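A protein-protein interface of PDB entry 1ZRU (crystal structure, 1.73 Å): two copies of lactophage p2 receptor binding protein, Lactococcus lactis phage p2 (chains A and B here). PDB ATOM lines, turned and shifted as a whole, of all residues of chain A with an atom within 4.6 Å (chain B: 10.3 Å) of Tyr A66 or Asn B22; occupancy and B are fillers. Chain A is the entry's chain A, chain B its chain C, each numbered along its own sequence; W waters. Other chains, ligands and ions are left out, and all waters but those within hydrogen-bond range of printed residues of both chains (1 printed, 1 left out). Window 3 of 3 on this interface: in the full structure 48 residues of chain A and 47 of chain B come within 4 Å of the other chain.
OE1 of Glu A68 lies within hydrogen-bond range of ND2 of Asn B22, at 2.9 Å.
OE1 of Glu A68 lies within salt-bridge range of NZ of Lys B25 (3.2 Å).
N of Phe A6 lies within hydrogen-bond range of O of Tyr A66.
The side-chain hydroxyl of Thr A7 sits at hydrogen-bond distance from the backbone NH of Tyr A66.
OG of Ser A59 is in hydrogen-bond range of OH of Tyr A66 (2.7 Å).
The side-chain hydroxyl (OH) of Tyr A66 lies within hydrogen-bond range of the side-chain carboxylate (OE1) of Glu A68 (2.5 Å).
The backbone NH (N) of Gly B19 lies within hydrogen-bond range of the side-chain amide oxygen (OD1) of Asn B22.
The side-chain amide oxygen (OD1) of Asn B22 sits close to the side-chain amide oxygen (OD1) of Asn B21, at 3.4 Å.
Phe A6 touches Asn B22.
SD of Met B29 touches CB of Ser A59 (3.5 Å).
Leu B26 touches Ile A61 (CD1 to CD1, 3.6 Å).
CB of Met B29 touches CD1 of Ile A61, 3.9 Å away.
Leu B30 touches Ile A61.
O of Asn B22 touches CZ of Tyr A66, 3.9 Å away.
Tyr A66 touches Lys B25 (OH to CB, 3.4 Å).
Tyr A66 touches Leu B26.
Tyr A66 touches Met B29.
No residue of chain B comes within 4 Å of Thr A7.
Ser A59 touches just one residue of chain B: Met B29 (3.5 Å).
No residue of chain B comes within 4 Å of Gly A64.
Of chain B, only Asn B22, Lys B25, Leu B26 and Met B29 come within 4 Å of Tyr A66.
No residue of chain B comes within 4 Å of Phe A67.
Asn B22 touches three residues of chain A.
Of the printed residues of chain A, Leu B26 touches Ile A61 and Tyr A66.
Of the printed residues of chain A, Leu B30 touches Ile A61 (3.7 Å).
The nearest residue of chain B that does not touch Tyr A66 is Asn B21 (5.2 Å).
Of the 25 printed residues of chain B, 5 touch a printed residue of chain A.
4 positions are printed for both chains.
Water W1 lies within hydrogen-bond range of OG of Ser A59 (2.8 Å), NZ of Lys B25 (2.9 Å) and OE1 of Glu A68 (3.3 Å).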
ATOM      1  N   ASN A   5      17.249  12.937  20.557  1.00  0.00           N
ATOM      2  CA  ASN A   5      17.798  12.828  21.906  1.00  0.00           C
ATOM      3  C   ASN A   5      16.928  13.515  22.940  1.00  0.00           C
ATOM      4  O   ASN A   5      16.337  14.569  22.676  1.00  0.00           O
ATOM      5  CB  ASN A   5      19.207  13.427  21.945  1.00  0.00           C
ATOM      6  CG  ASN A   5      20.156  12.742  20.982  1.00  0.00           C
ATOM      7  OD1 ASN A   5      20.676  13.366  20.054  1.00  0.00           O
ATOM      8  ND2 ASN A   5      20.360  11.439  21.178  1.00  0.00           N
ATOM      9  N   PHE A   6      16.872  12.929  24.129  1.00  0.00           N
ATOM     10  CA  PHE A   6      15.963  13.405  25.159  1.00  0.00           C
ATOM     11  C   PHE A   6      16.687  13.558  26.494  1.00  0.00           C
ATOM     12  O   PHE A   6      16.678  14.648  27.079  1.00  0.00           O
ATOM     13  CB  PHE A   6      14.745  12.470  25.275  1.00  0.00           C
ATOM     14  CG  PHE A   6      13.944  12.357  23.993  1.00  0.00           C
ATOM     15  CD1 PHE A   6      14.217  11.353  23.069  1.00  0.00           C
ATOM     16  CD2 PHE A   6      12.933  13.275  23.703  1.00  0.00           C
ATOM     17  CE1 PHE A   6      13.485  11.254  21.873  1.00  0.00           C
ATOM     18  CE2 PHE A   6      12.203  13.184  22.514  1.00  0.00           C
ATOM     19  CZ  PHE A   6      12.484  12.167  21.600  1.00  0.00           C
ATOM     20  N   THR A   7      17.328  12.480  26.956  1.00  0.00           N
ATOM     21  CA  THR A   7      18.049  12.481  28.241  1.00  0.00           C
ATOM     22  C   THR A   7      19.411  13.171  28.087  1.00  0.00           C
ATOM     23  O   THR A   7      20.446  12.622  28.465  1.00  0.00           O
ATOM     24  CB  THR A   7      18.252  11.038  28.786  1.00  0.00           C
ATOM     25  OG1 THR A   7      17.133  10.232  28.437  1.00  0.00           O
ATOM     26  CG2 THR A   7      18.388  11.021  30.315  1.00  0.00           C
ATOM     27  N   PHE A   8      19.400  14.373  27.516  1.00  0.00           N
ATOM     28  CA  PHE A   8      20.638  15.108  27.240  1.00  0.00           C
ATOM     29  C   PHE A   8      20.427  16.592  27.510  1.00  0.00           C
ATOM     30  O   PHE A   8      19.379  17.141  27.157  1.00  0.00           O
ATOM     31  CB  PHE A   8      21.087  14.904  25.782  1.00  0.00           C
ATOM     32  CG  PHE A   8      21.370  13.465  25.419  1.00  0.00           C
ATOM     33  CD1 PHE A   8      20.363  12.654  24.894  1.00  0.00           C
ATOM     34  CD2 PHE A   8      22.637  12.929  25.591  1.00  0.00           C
ATOM     35  CE1 PHE A   8      20.614  11.323  24.552  1.00  0.00           C
ATOM     36  CE2 PHE A   8      22.908  11.599  25.250  1.00  0.00           C
ATOM     37  CZ  PHE A   8      21.892  10.795  24.726  1.00  0.00           C
ATOM     38  N   SER A  59      13.711   2.682  19.949  1.00  0.00           N
ATOM     39  CA  SER A  59      14.243   3.412  21.102  1.00  0.00           C
ATOM     40  C   SER A  59      15.393   2.637  21.718  1.00  0.00           C
ATOM     41  O   SER A  59      15.393   1.392  21.731  1.00  0.00           O
ATOM     42  CB  SER A  59      13.174   3.585  22.204  1.00  0.00           C
ATOM     43  OG  SER A  59      12.056   4.355  21.792  1.00  0.00           O
ATOM     44  N   ILE A  60      16.372   3.377  22.228  1.00  0.00           N
ATOM     45  CA  ILE A  60      17.502   2.783  22.917  1.00  0.00           C
ATOM     46  C   ILE A  60      17.775   3.583  24.199  1.00  0.00           C
ATOM     47  O   ILE A  60      17.620   4.810  24.213  1.00  0.00           O
ATOM     48  CB  ILE A  60      18.778   2.801  22.026  1.00  0.00           C
ATOM     49  CG1 ILE A  60      18.607   1.876  20.808  1.00  0.00           C
ATOM     50  CG2 ILE A  60      20.009   2.316  22.829  1.00  0.00           C
ATOM     51  CD1 ILE A  60      19.641   2.102  19.723  1.00  0.00           C
ATOM     52  N   ILE A  61      18.169   2.875  25.255  1.00  0.00           N
ATOM     53  CA  ILE A  61      18.744   3.500  26.455  1.00  0.00           C
ATOM     54  C   ILE A  61      20.156   2.957  26.573  1.00  0.00           C
ATOM     55  O   ILE A  61      20.379   1.738  26.582  1.00  0.00           O
ATOM     56  CB  ILE A  61      17.959   3.179  27.757  1.00  0.00           C
ATOM     57  CG1 ILE A  61      16.495   3.590  27.594  1.00  0.00           C
ATOM     58  CG2 ILE A  61      18.614   3.886  28.958  1.00  0.00           C
ATOM     59  CD1 ILE A  61      15.581   3.105  28.722  1.00  0.00           C
ATOM     60  N   GLY A  64      21.976   5.054  30.652  1.00  0.00           N
ATOM     61  CA  GLY A  64      20.822   5.755  31.227  1.00  0.00           C
ATOM     62  C   GLY A  64      20.319   6.923  30.384  1.00  0.00           C
ATOM     63  O   GLY A  64      19.478   7.688  30.848  1.00  0.00           O
ATOM     64  N   ARG A  65      20.837   7.046  29.157  1.00  0.00           N
ATOM     65  CA  ARG A  65      20.399   8.087  28.218  1.00  0.00           C
ATOM     66  C   ARG A  65      19.449   7.492  27.179  1.00  0.00           C
ATOM     67  O   ARG A  65      19.796   6.521  26.496  1.00  0.00           O
ATOM     68  CB  ARG A  65      21.592   8.765  27.527  1.00  0.00           C
ATOM     69  CG  ARG A  65      22.693   9.263  28.475  1.00  0.00           C
ATOM     70  CD  ARG A  65      22.149  10.050  29.662  1.00  0.00           C
ATOM     71  NE  ARG A  65      23.229  10.644  30.465  1.00  0.00           N
ATOM     72  CZ  ARG A  65      23.722  11.870  30.285  1.00  0.00           C
ATOM     73  NH1 ARG A  65      23.242  12.670  29.327  1.00  0.00           N
ATOM     74  NH2 ARG A  65      24.702  12.308  31.073  1.00  0.00           N
ATOM     75  N   TYR A  66      18.268   8.097  27.056  1.00  0.00           N
ATOM     76  CA  TYR A  66      17.213   7.611  26.147  1.00  0.00           C
ATOM     77  C   TYR A  66      17.253   8.386  24.835  1.00  0.00           C
ATOM     78  O   TYR A  66      17.329   9.622  24.841  1.00  0.00           O
ATOM     79  CB  TYR A  66      15.828   7.778  26.806  1.00  0.00           C
ATOM     80  CG  TYR A  66      14.656   7.458  25.900  1.00  0.00           C
ATOM     81  CD1 TYR A  66      14.132   6.167  25.846  1.00  0.00           C
ATOM     82  CD2 TYR A  66      14.084   8.439  25.076  1.00  0.00           C
ATOM     83  CE1 TYR A  66      13.062   5.848  25.001  1.00  0.00           C
ATOM     84  CE2 TYR A  66      13.002   8.140  24.226  1.00  0.00           C
ATOM     85  CZ  TYR A  66      12.512   6.838  24.176  1.00  0.00           C
ATOM     86  OH  TYR A  66      11.471   6.522  23.349  1.00  0.00           O
ATOM     87  N   PHE A  67      17.195   7.668  23.719  1.00  0.00           N
ATOM     88  CA  PHE A  67      17.096   8.329  22.409  1.00  0.00           C
ATOM     89  C   PHE A  67      16.327   7.446  21.434  1.00  0.00           C
ATOM     90  O   PHE A  67      16.116   6.259  21.694  1.00  0.00           O
ATOM     91  CB  PHE A  67      18.477   8.702  21.846  1.00  0.00           C
ATOM     92  CG  PHE A  67      19.454   7.565  21.818  1.00  0.00           C
ATOM     93  CD1 PHE A  67      19.639   6.801  20.664  1.00  0.00           C
ATOM     94  CD2 PHE A  67      20.211   7.270  22.958  1.00  0.00           C
ATOM     95  CE1 PHE A  67      20.557   5.728  20.665  1.00  0.00           C
ATOM     96  CE2 PHE A  67      21.122   6.210  22.965  1.00  0.00           C
ATOM     97  CZ  PHE A  67      21.293   5.446  21.821  1.00  0.00           C
ATOM     98  N   GLU A  68      15.887   8.036  20.318  1.00  0.00           N
ATOM     99  CA  GLU A  68      15.056   7.340  19.353  1.00  0.00           C
ATOM    100  C   GLU A  68      15.687   7.393  17.968  1.00  0.00           C
ATOM    101  O   GLU A  68      16.174   8.440  17.549  1.00  0.00           O
ATOM    102  CB  GLU A  68      13.655   7.963  19.291  1.00  0.00           C
ATOM    103  CG  GLU A  68      12.927   7.841  20.642  1.00  0.00           C
ATOM    104  CD  GLU A  68      11.562   8.512  20.681  1.00  0.00           C
ATOM    105  OE1 GLU A  68      10.863   8.316  21.696  1.00  0.00           O
ATOM    106  OE2 GLU A  68      11.187   9.242  19.722  1.00  0.00           O
ATOM    107  N   THR B   7       1.452  11.318  33.693  1.00  0.00           N
ATOM    108  CA  THR B   7       2.227  11.194  32.438  1.00  0.00           C
ATOM    109  C   THR B   7       1.360  11.483  31.207  1.00  0.00           C
ATOM    110  O   THR B   7       1.182  10.625  30.342  1.00  0.00           O
ATOM    111  CB  THR B   7       2.878   9.778  32.307  1.00  0.00           C
ATOM    112  OG1 THR B   7       3.180   9.267  33.609  1.00  0.00           O
ATOM    113  CG2 THR B   7       4.169   9.828  31.462  1.00  0.00           C
ATOM    114  N   PHE B   8       0.808  12.696  31.131  1.00  0.00           N
ATOM    115  CA  PHE B   8      -0.094  13.053  30.033  1.00  0.00           C
ATOM    116  C   PHE B   8       0.077  14.515  29.658  1.00  0.00           C
ATOM    117  O   PHE B   8       0.260  15.355  30.540  1.00  0.00           O
ATOM    118  CB  PHE B   8      -1.559  12.805  30.425  1.00  0.00           C
ATOM    119  CG  PHE B   8      -1.879  11.359  30.715  1.00  0.00           C
ATOM    120  CD1 PHE B   8      -1.671  10.824  31.988  1.00  0.00           C
ATOM    121  CD2 PHE B   8      -2.360  10.529  29.712  1.00  0.00           C
ATOM    122  CE1 PHE B   8      -1.952   9.486  32.264  1.00  0.00           C
ATOM    123  CE2 PHE B   8      -2.647   9.182  29.976  1.00  0.00           C
ATOM    124  CZ  PHE B   8      -2.441   8.664  31.255  1.00  0.00           C
ATOM    125  N   PHE B   9       0.017  14.798  28.356  1.00  0.00           N
ATOM    126  CA  PHE B   9      -0.041  16.172  27.830  1.00  0.00           C
ATOM    127  C   PHE B   9       1.026  17.104  28.415  1.00  0.00           C
ATOM    128  O   PHE B   9       2.207  16.742  28.483  1.00  0.00           O
ATOM    129  CB  PHE B   9      -1.444  16.759  28.044  1.00  0.00           C
ATOM    130  CG  PHE B   9      -2.564  15.793  27.715  1.00  0.00           C
ATOM    131  CD1 PHE B   9      -3.497  15.432  28.682  1.00  0.00           C
ATOM    132  CD2 PHE B   9      -2.666  15.221  26.440  1.00  0.00           C
ATOM    133  CE1 PHE B   9      -4.524  14.533  28.386  1.00  0.00           C
ATOM    134  CE2 PHE B   9      -3.698  14.316  26.136  1.00  0.00           C
ATOM    135  CZ  PHE B   9      -4.623  13.978  27.111  1.00  0.00           C
ATOM    136  N   GLY B  19       8.400  14.779  25.426  1.00  0.00           N
ATOM    137  CA  GLY B  19       6.966  14.488  25.409  1.00  0.00           C
ATOM    138  C   GLY B  19       6.578  13.408  26.407  1.00  0.00           C
ATOM    139  O   GLY B  19       7.431  12.649  26.889  1.00  0.00           O
ATOM    140  N   SER B  20       5.286  13.348  26.727  1.00  0.00           N
ATOM    141  CA  SER B  20       4.767  12.295  27.577  1.00  0.00           C
ATOM    142  C   SER B  20       4.926  10.939  26.882  1.00  0.00           C
ATOM    143  O   SER B  20       5.103   9.929  27.561  1.00  0.00           O
ATOM    144  CB  SER B  20       3.300  12.551  27.941  1.00  0.00           C
ATOM    145  OG  SER B  20       3.195  13.711  28.742  1.00  0.00           O
ATOM    146  N   ASN B  21       4.872  10.913  25.545  1.00  0.00           N
ATOM    147  CA  ASN B  21       5.023   9.631  24.843  1.00  0.00           C
ATOM    148  C   ASN B  21       6.463   9.116  24.925  1.00  0.00           C
ATOM    149  O   ASN B  21       6.699   7.904  25.046  1.00  0.00           O
ATOM    150  CB  ASN B  21       4.508   9.693  23.399  1.00  0.00           C
ATOM    151  CG  ASN B  21       5.289  10.643  22.545  1.00  0.00           C
ATOM    152  OD1 ASN B  21       5.595  11.764  22.963  1.00  0.00           O
ATOM    153  ND2 ASN B  21       5.623  10.208  21.331  1.00  0.00           N
ATOM    154  N   ASN B  22       7.426  10.031  24.909  1.00  0.00           N
ATOM    155  CA  ASN B  22       8.826   9.638  25.060  1.00  0.00           C
ATOM    156  C   ASN B  22       9.116   9.137  26.467  1.00  0.00           C
ATOM    157  O   ASN B  22       9.817   8.145  26.638  1.00  0.00           O
ATOM    158  CB  ASN B  22       9.754  10.795  24.701  1.00  0.00           C
ATOM    159  CG  ASN B  22       9.343  11.471  23.410  1.00  0.00           C
ATOM    160  OD1 ASN B  22       8.901  12.634  23.409  1.00  0.00           O
ATOM    161  ND2 ASN B  22       9.428  10.730  22.307  1.00  0.00           N
ATOM    162  N   ASP B  23       8.568   9.816  27.473  1.00  0.00           N
ATOM    163  CA  ASP B  23       8.707   9.311  28.840  1.00  0.00           C
ATOM    164  C   ASP B  23       7.979   7.981  29.015  1.00  0.00           C
ATOM    165  O   ASP B  23       8.513   7.084  29.674  1.00  0.00           O
ATOM    166  CB  ASP B  23       8.272  10.356  29.872  1.00  0.00           C
ATOM    167  CG  ASP B  23       9.356  11.420  30.095  1.00  0.00           C
ATOM    168  OD1 ASP B  23      10.531  11.181  29.717  1.00  0.00           O
ATOM    169  OD2 ASP B  23       9.041  12.483  30.656  1.00  0.00           O
ATOM    170  N   GLY B  24       6.795   7.852  28.407  1.00  0.00           N
ATOM    171  CA  GLY B  24       6.055   6.566  28.433  1.00  0.00           C
ATOM    172  C   GLY B  24       6.932   5.431  27.932  1.00  0.00           C
ATOM    173  O   GLY B  24       7.059   4.390  28.577  1.00  0.00           O
ATOM    174  N   LYS B  25       7.554   5.630  26.770  1.00  0.00           N
ATOM    175  CA  LYS B  25       8.401   4.580  26.197  1.00  0.00           C
ATOM    176  C   LYS B  25       9.617   4.277  27.083  1.00  0.00           C
ATOM    177  O   LYS B  25       9.942   3.108  27.320  1.00  0.00           O
ATOM    178  CB  LYS B  25       8.805   4.957  24.770  1.00  0.00           C
ATOM    179  CG  LYS B  25       7.615   4.873  23.823  1.00  0.00           C
ATOM    180  CD  LYS B  25       7.977   5.206  22.370  1.00  0.00           C
ATOM    181  CE  LYS B  25       7.972   6.685  22.098  1.00  0.00           C
ATOM    182  NZ  LYS B  25       8.229   6.932  20.622  1.00  0.00           N
ATOM    183  N   LEU B  26      10.251   5.332  27.593  1.00  0.00           N
ATOM    184  CA  LEU B  26      11.388   5.214  28.504  1.00  0.00           C
ATOM    185  C   LEU B  26      10.982   4.342  29.704  1.00  0.00           C
ATOM    186  O   LEU B  26      11.685   3.379  30.044  1.00  0.00           O
ATOM    187  CB  LEU B  26      11.833   6.613  28.973  1.00  0.00           C
ATOM    188  CG  LEU B  26      12.684   6.692  30.247  1.00  0.00           C
ATOM    189  CD1 LEU B  26      14.073   6.104  30.088  1.00  0.00           C
ATOM    190  CD2 LEU B  26      12.742   8.165  30.770  1.00  0.00           C
ATOM    191  N   TYR B  27       9.829   4.656  30.303  1.00  0.00           N
ATOM    192  CA  TYR B  27       9.403   3.951  31.525  1.00  0.00           C
ATOM    193  C   TYR B  27       9.088   2.482  31.230  1.00  0.00           C
ATOM    194  O   TYR B  27       9.488   1.579  31.991  1.00  0.00           O
ATOM    195  CB  TYR B  27       8.218   4.641  32.195  1.00  0.00           C
ATOM    196  CG  TYR B  27       8.523   6.056  32.650  1.00  0.00           C
ATOM    197  CD1 TYR B  27       9.815   6.430  33.038  1.00  0.00           C
ATOM    198  CD2 TYR B  27       7.512   7.015  32.685  1.00  0.00           C
ATOM    199  CE1 TYR B  27      10.101   7.768  33.450  1.00  0.00           C
ATOM    200  CE2 TYR B  27       7.784   8.331  33.089  1.00  0.00           C
ATOM    201  CZ  TYR B  27       9.062   8.688  33.457  1.00  0.00           C
ATOM    202  OH  TYR B  27       9.291   9.988  33.849  1.00  0.00           O
ATOM    203  N   MET B  28       8.432   2.241  30.099  1.00  0.00           N
ATOM    204  CA  MET B  28       8.138   0.852  29.695  1.00  0.00           C
ATOM    205  C   MET B  28       9.425   0.051  29.546  1.00  0.00           C
ATOM    206  O   MET B  28       9.495  -1.113  29.954  1.00  0.00           O
ATOM    207  CB  MET B  28       7.357   0.823  28.387  1.00  0.00           C
ATOM    208  CG  MET B  28       5.903   1.301  28.529  1.00  0.00           C
ATOM    209  SD  MET B  28       5.064   1.369  26.935  1.00  0.00           S
ATOM    210  CE  MET B  28       4.745  -0.380  26.677  1.00  0.00           C
ATOM    211  N   MET B  29      10.442   0.677  28.952  1.00  0.00           N
ATOM    212  CA  MET B  29      11.733   0.020  28.746  1.00  0.00           C
ATOM    213  C   MET B  29      12.476  -0.251  30.044  1.00  0.00           C
ATOM    214  O   MET B  29      13.040  -1.326  30.207  1.00  0.00           O
ATOM    215  CB  MET B  29      12.592   0.804  27.767  1.00  0.00           C
ATOM    216  CG  MET B  29      11.955   0.794  26.369  1.00  0.00           C
ATOM    217  SD  MET B  29      12.791   1.945  25.245  1.00  0.00           S
ATOM    218  CE  MET B  29      14.398   1.126  25.054  1.00  0.00           C
ATOM    219  N   LEU B  30      12.471   0.714  30.955  1.00  0.00           N
ATOM    220  CA  LEU B  30      13.169   0.543  32.238  1.00  0.00           C
ATOM    221  C   LEU B  30      12.575  -0.627  33.044  1.00  0.00           C
ATOM    222  O   LEU B  30      13.315  -1.421  33.660  1.00  0.00           O
ATOM    223  CB  LEU B  30      13.079   1.842  33.049  1.00  0.00           C
ATOM    224  CG  LEU B  30      13.887   3.038  32.509  1.00  0.00           C
ATOM    225  CD1 LEU B  30      13.559   4.282  33.383  1.00  0.00           C
ATOM    226  CD2 LEU B  30      15.418   2.798  32.425  1.00  0.00           C
ATOM    227  N   TYR B  35       2.524  -3.380  26.198  1.00  0.00           N
ATOM    228  CA  TYR B  35       1.210  -2.737  26.318  1.00  0.00           C
ATOM    229  C   TYR B  35       0.124  -3.650  26.868  1.00  0.00           C
ATOM    230  O   TYR B  35      -1.018  -3.211  27.075  1.00  0.00           O
ATOM    231  CB  TYR B  35       0.762  -2.148  24.969  1.00  0.00           C
ATOM    232  CG  TYR B  35       1.568  -0.935  24.581  1.00  0.00           C
ATOM    233  CD1 TYR B  35       1.379   0.285  25.242  1.00  0.00           C
ATOM    234  CD2 TYR B  35       2.538  -1.004  23.563  1.00  0.00           C
ATOM    235  CE1 TYR B  35       2.120   1.406  24.894  1.00  0.00           C
ATOM    236  CE2 TYR B  35       3.278   0.121  23.205  1.00  0.00           C
ATOM    237  CZ  TYR B  35       3.057   1.318  23.878  1.00  0.00           C
ATOM    238  OH  TYR B  35       3.785   2.434  23.542  1.00  0.00           O
ATOM    239  N   GLY B  63       0.982   1.343  29.665  1.00  0.00           N
ATOM    240  CA  GLY B  63       1.672   1.956  28.518  1.00  0.00           C
ATOM    241  C   GLY B  63       2.689   3.010  28.922  1.00  0.00           C
ATOM    242  O   GLY B  63       2.880   4.012  28.220  1.00  0.00           O
ATOM    243  N   GLY B  64       3.323   2.798  30.073  1.00  0.00           N
ATOM    244  CA  GLY B  64       4.322   3.711  30.610  1.00  0.00           C
ATOM    245  C   GLY B  64       3.741   4.996  31.187  1.00  0.00           C
ATOM    246  O   GLY B  64       4.501   5.868  31.605  1.00  0.00           O
ATOM    247  N   ARG B  65       2.412   5.089  31.234  1.00  0.00           N
ATOM    248  CA  ARG B  65       1.733   6.284  31.765  1.00  0.00           C
ATOM    249  C   ARG B  65       1.293   6.028  33.199  1.00  0.00           C
ATOM    250  O   ARG B  65       0.561   5.071  33.465  1.00  0.00           O
ATOM    251  CB  ARG B  65       0.516   6.686  30.914  1.00  0.00           C
ATOM    252  CG  ARG B  65       0.794   6.820  29.397  1.00  0.00           C
ATOM    253  CD  ARG B  65       1.937   7.755  29.079  1.00  0.00           C
ATOM    254  NE  ARG B  65       2.009   7.986  27.626  1.00  0.00           N
ATOM    255  CZ  ARG B  65       1.464   9.021  26.992  1.00  0.00           C
ATOM    256  NH1 ARG B  65       0.793   9.974  27.667  1.00  0.00           N
ATOM    257  NH2 ARG B  65       1.604   9.108  25.669  1.00  0.00           N
ATOM    258  N   LEU B  90      -6.042   9.284  24.536  1.00  0.00           N
ATOM    259  CA  LEU B  90      -5.362  10.568  24.613  1.00  0.00           C
ATOM    260  C   LEU B  90      -6.131  11.677  23.885  1.00  0.00           C
ATOM    261  O   LEU B  90      -5.838  12.851  24.085  1.00  0.00           O
ATOM    262  CB  LEU B  90      -3.914  10.452  24.117  1.00  0.00           C
ATOM    263  CG  LEU B  90      -3.010   9.466  24.881  1.00  0.00           C
ATOM    264  CD1 LEU B  90      -1.613   9.395  24.244  1.00  0.00           C
ATOM    265  CD2 LEU B  90      -2.910   9.807  26.365  1.00  0.00           C
ATOM    266  N   ASP B 111      -0.681   0.597  20.896  1.00  0.00           N
ATOM    267  CA  ASP B 111       0.519   1.412  21.134  1.00  0.00           C
ATOM    268  C   ASP B 111       0.211   2.912  21.168  1.00  0.00           C
ATOM    269  O   ASP B 111       0.313   3.610  20.148  1.00  0.00           O
ATOM    270  CB  ASP B 111       1.575   1.094  20.064  1.00  0.00           C
ATOM    271  CG  ASP B 111       2.918   1.807  20.304  1.00  0.00           C
ATOM    272  OD1 ASP B 111       3.013   2.789  21.100  1.00  0.00           O
ATOM    273  OD2 ASP B 111       3.891   1.359  19.667  1.00  0.00           O
ATOM    274  N   ILE B 112      -0.143   3.409  22.349  1.00  0.00           N
ATOM    275  CA  ILE B 112      -0.541   4.820  22.504  1.00  0.00           C
ATOM    276  C   ILE B 112       0.624   5.801  22.525  1.00  0.00           C
ATOM    277  O   ILE B 112       0.404   7.028  22.490  1.00  0.00           O
ATOM    278  CB  ILE B 112      -1.435   5.048  23.755  1.00  0.00           C
ATOM    279  CG1 ILE B 112      -0.733   4.549  25.032  1.00  0.00           C
ATOM    280  CG2 ILE B 112      -2.781   4.354  23.540  1.00  0.00           C
ATOM    281  CD1 ILE B 112      -1.370   5.061  26.308  1.00  0.00           C
ATOM    282  N   ASN B 113       1.856   5.302  22.594  1.00  0.00           N
ATOM    283  CA  ASN B 113       3.005   6.205  22.574  1.00  0.00           C
ATOM    284  C   ASN B 113       3.548   6.471  21.170  1.00  0.00           C
ATOM    285  O   ASN B 113       4.392   7.357  20.992  1.00  0.00           O
ATOM    286  CB  ASN B 113       4.123   5.702  23.487  1.00  0.00           C
ATOM    287  CG  ASN B 113       3.702   5.682  24.935  1.00  0.00           C
ATOM    288  OD1 ASN B 113       3.190   6.672  25.446  1.00  0.00           O
ATOM    289  ND2 ASN B 113       3.900   4.543  25.600  1.00  0.00           N
ATOM    290  N   ASN B 114       3.069   5.716  20.195  1.00  0.00           N
ATOM    291  CA  ASN B 114       3.532   5.863  18.798  1.00  0.00           C
ATOM    292  C   ASN B 114       2.440   6.097  17.768  1.00  0.00           C
ATOM    293  O   ASN B 114       2.720   6.226  16.568  1.00  0.00           O
ATOM    294  CB  ASN B 114       4.329   4.644  18.377  1.00  0.00           C
ATOM    295  CG  ASN B 114       5.646   4.558  19.086  1.00  0.00           C
ATOM    296  OD1 ASN B 114       6.446   5.502  19.050  1.00  0.00           O
ATOM    297  ND2 ASN B 114       5.887   3.419  19.750  1.00  0.00           N
ATOM    298  N   GLY B 115       1.193   6.108  18.219  1.00  0.00           N
ATOM    299  CA  GLY B 115       0.072   6.236  17.294  1.00  0.00           C
ATOM    300  C   GLY B 115      -1.210   6.489  18.036  1.00  0.00           C
ATOM    301  O   GLY B 115      -1.234   6.533  19.274  1.00  0.00           O
HETATM  302  O   HOH W   1      10.649   5.640  19.721  1.00  0.00           O
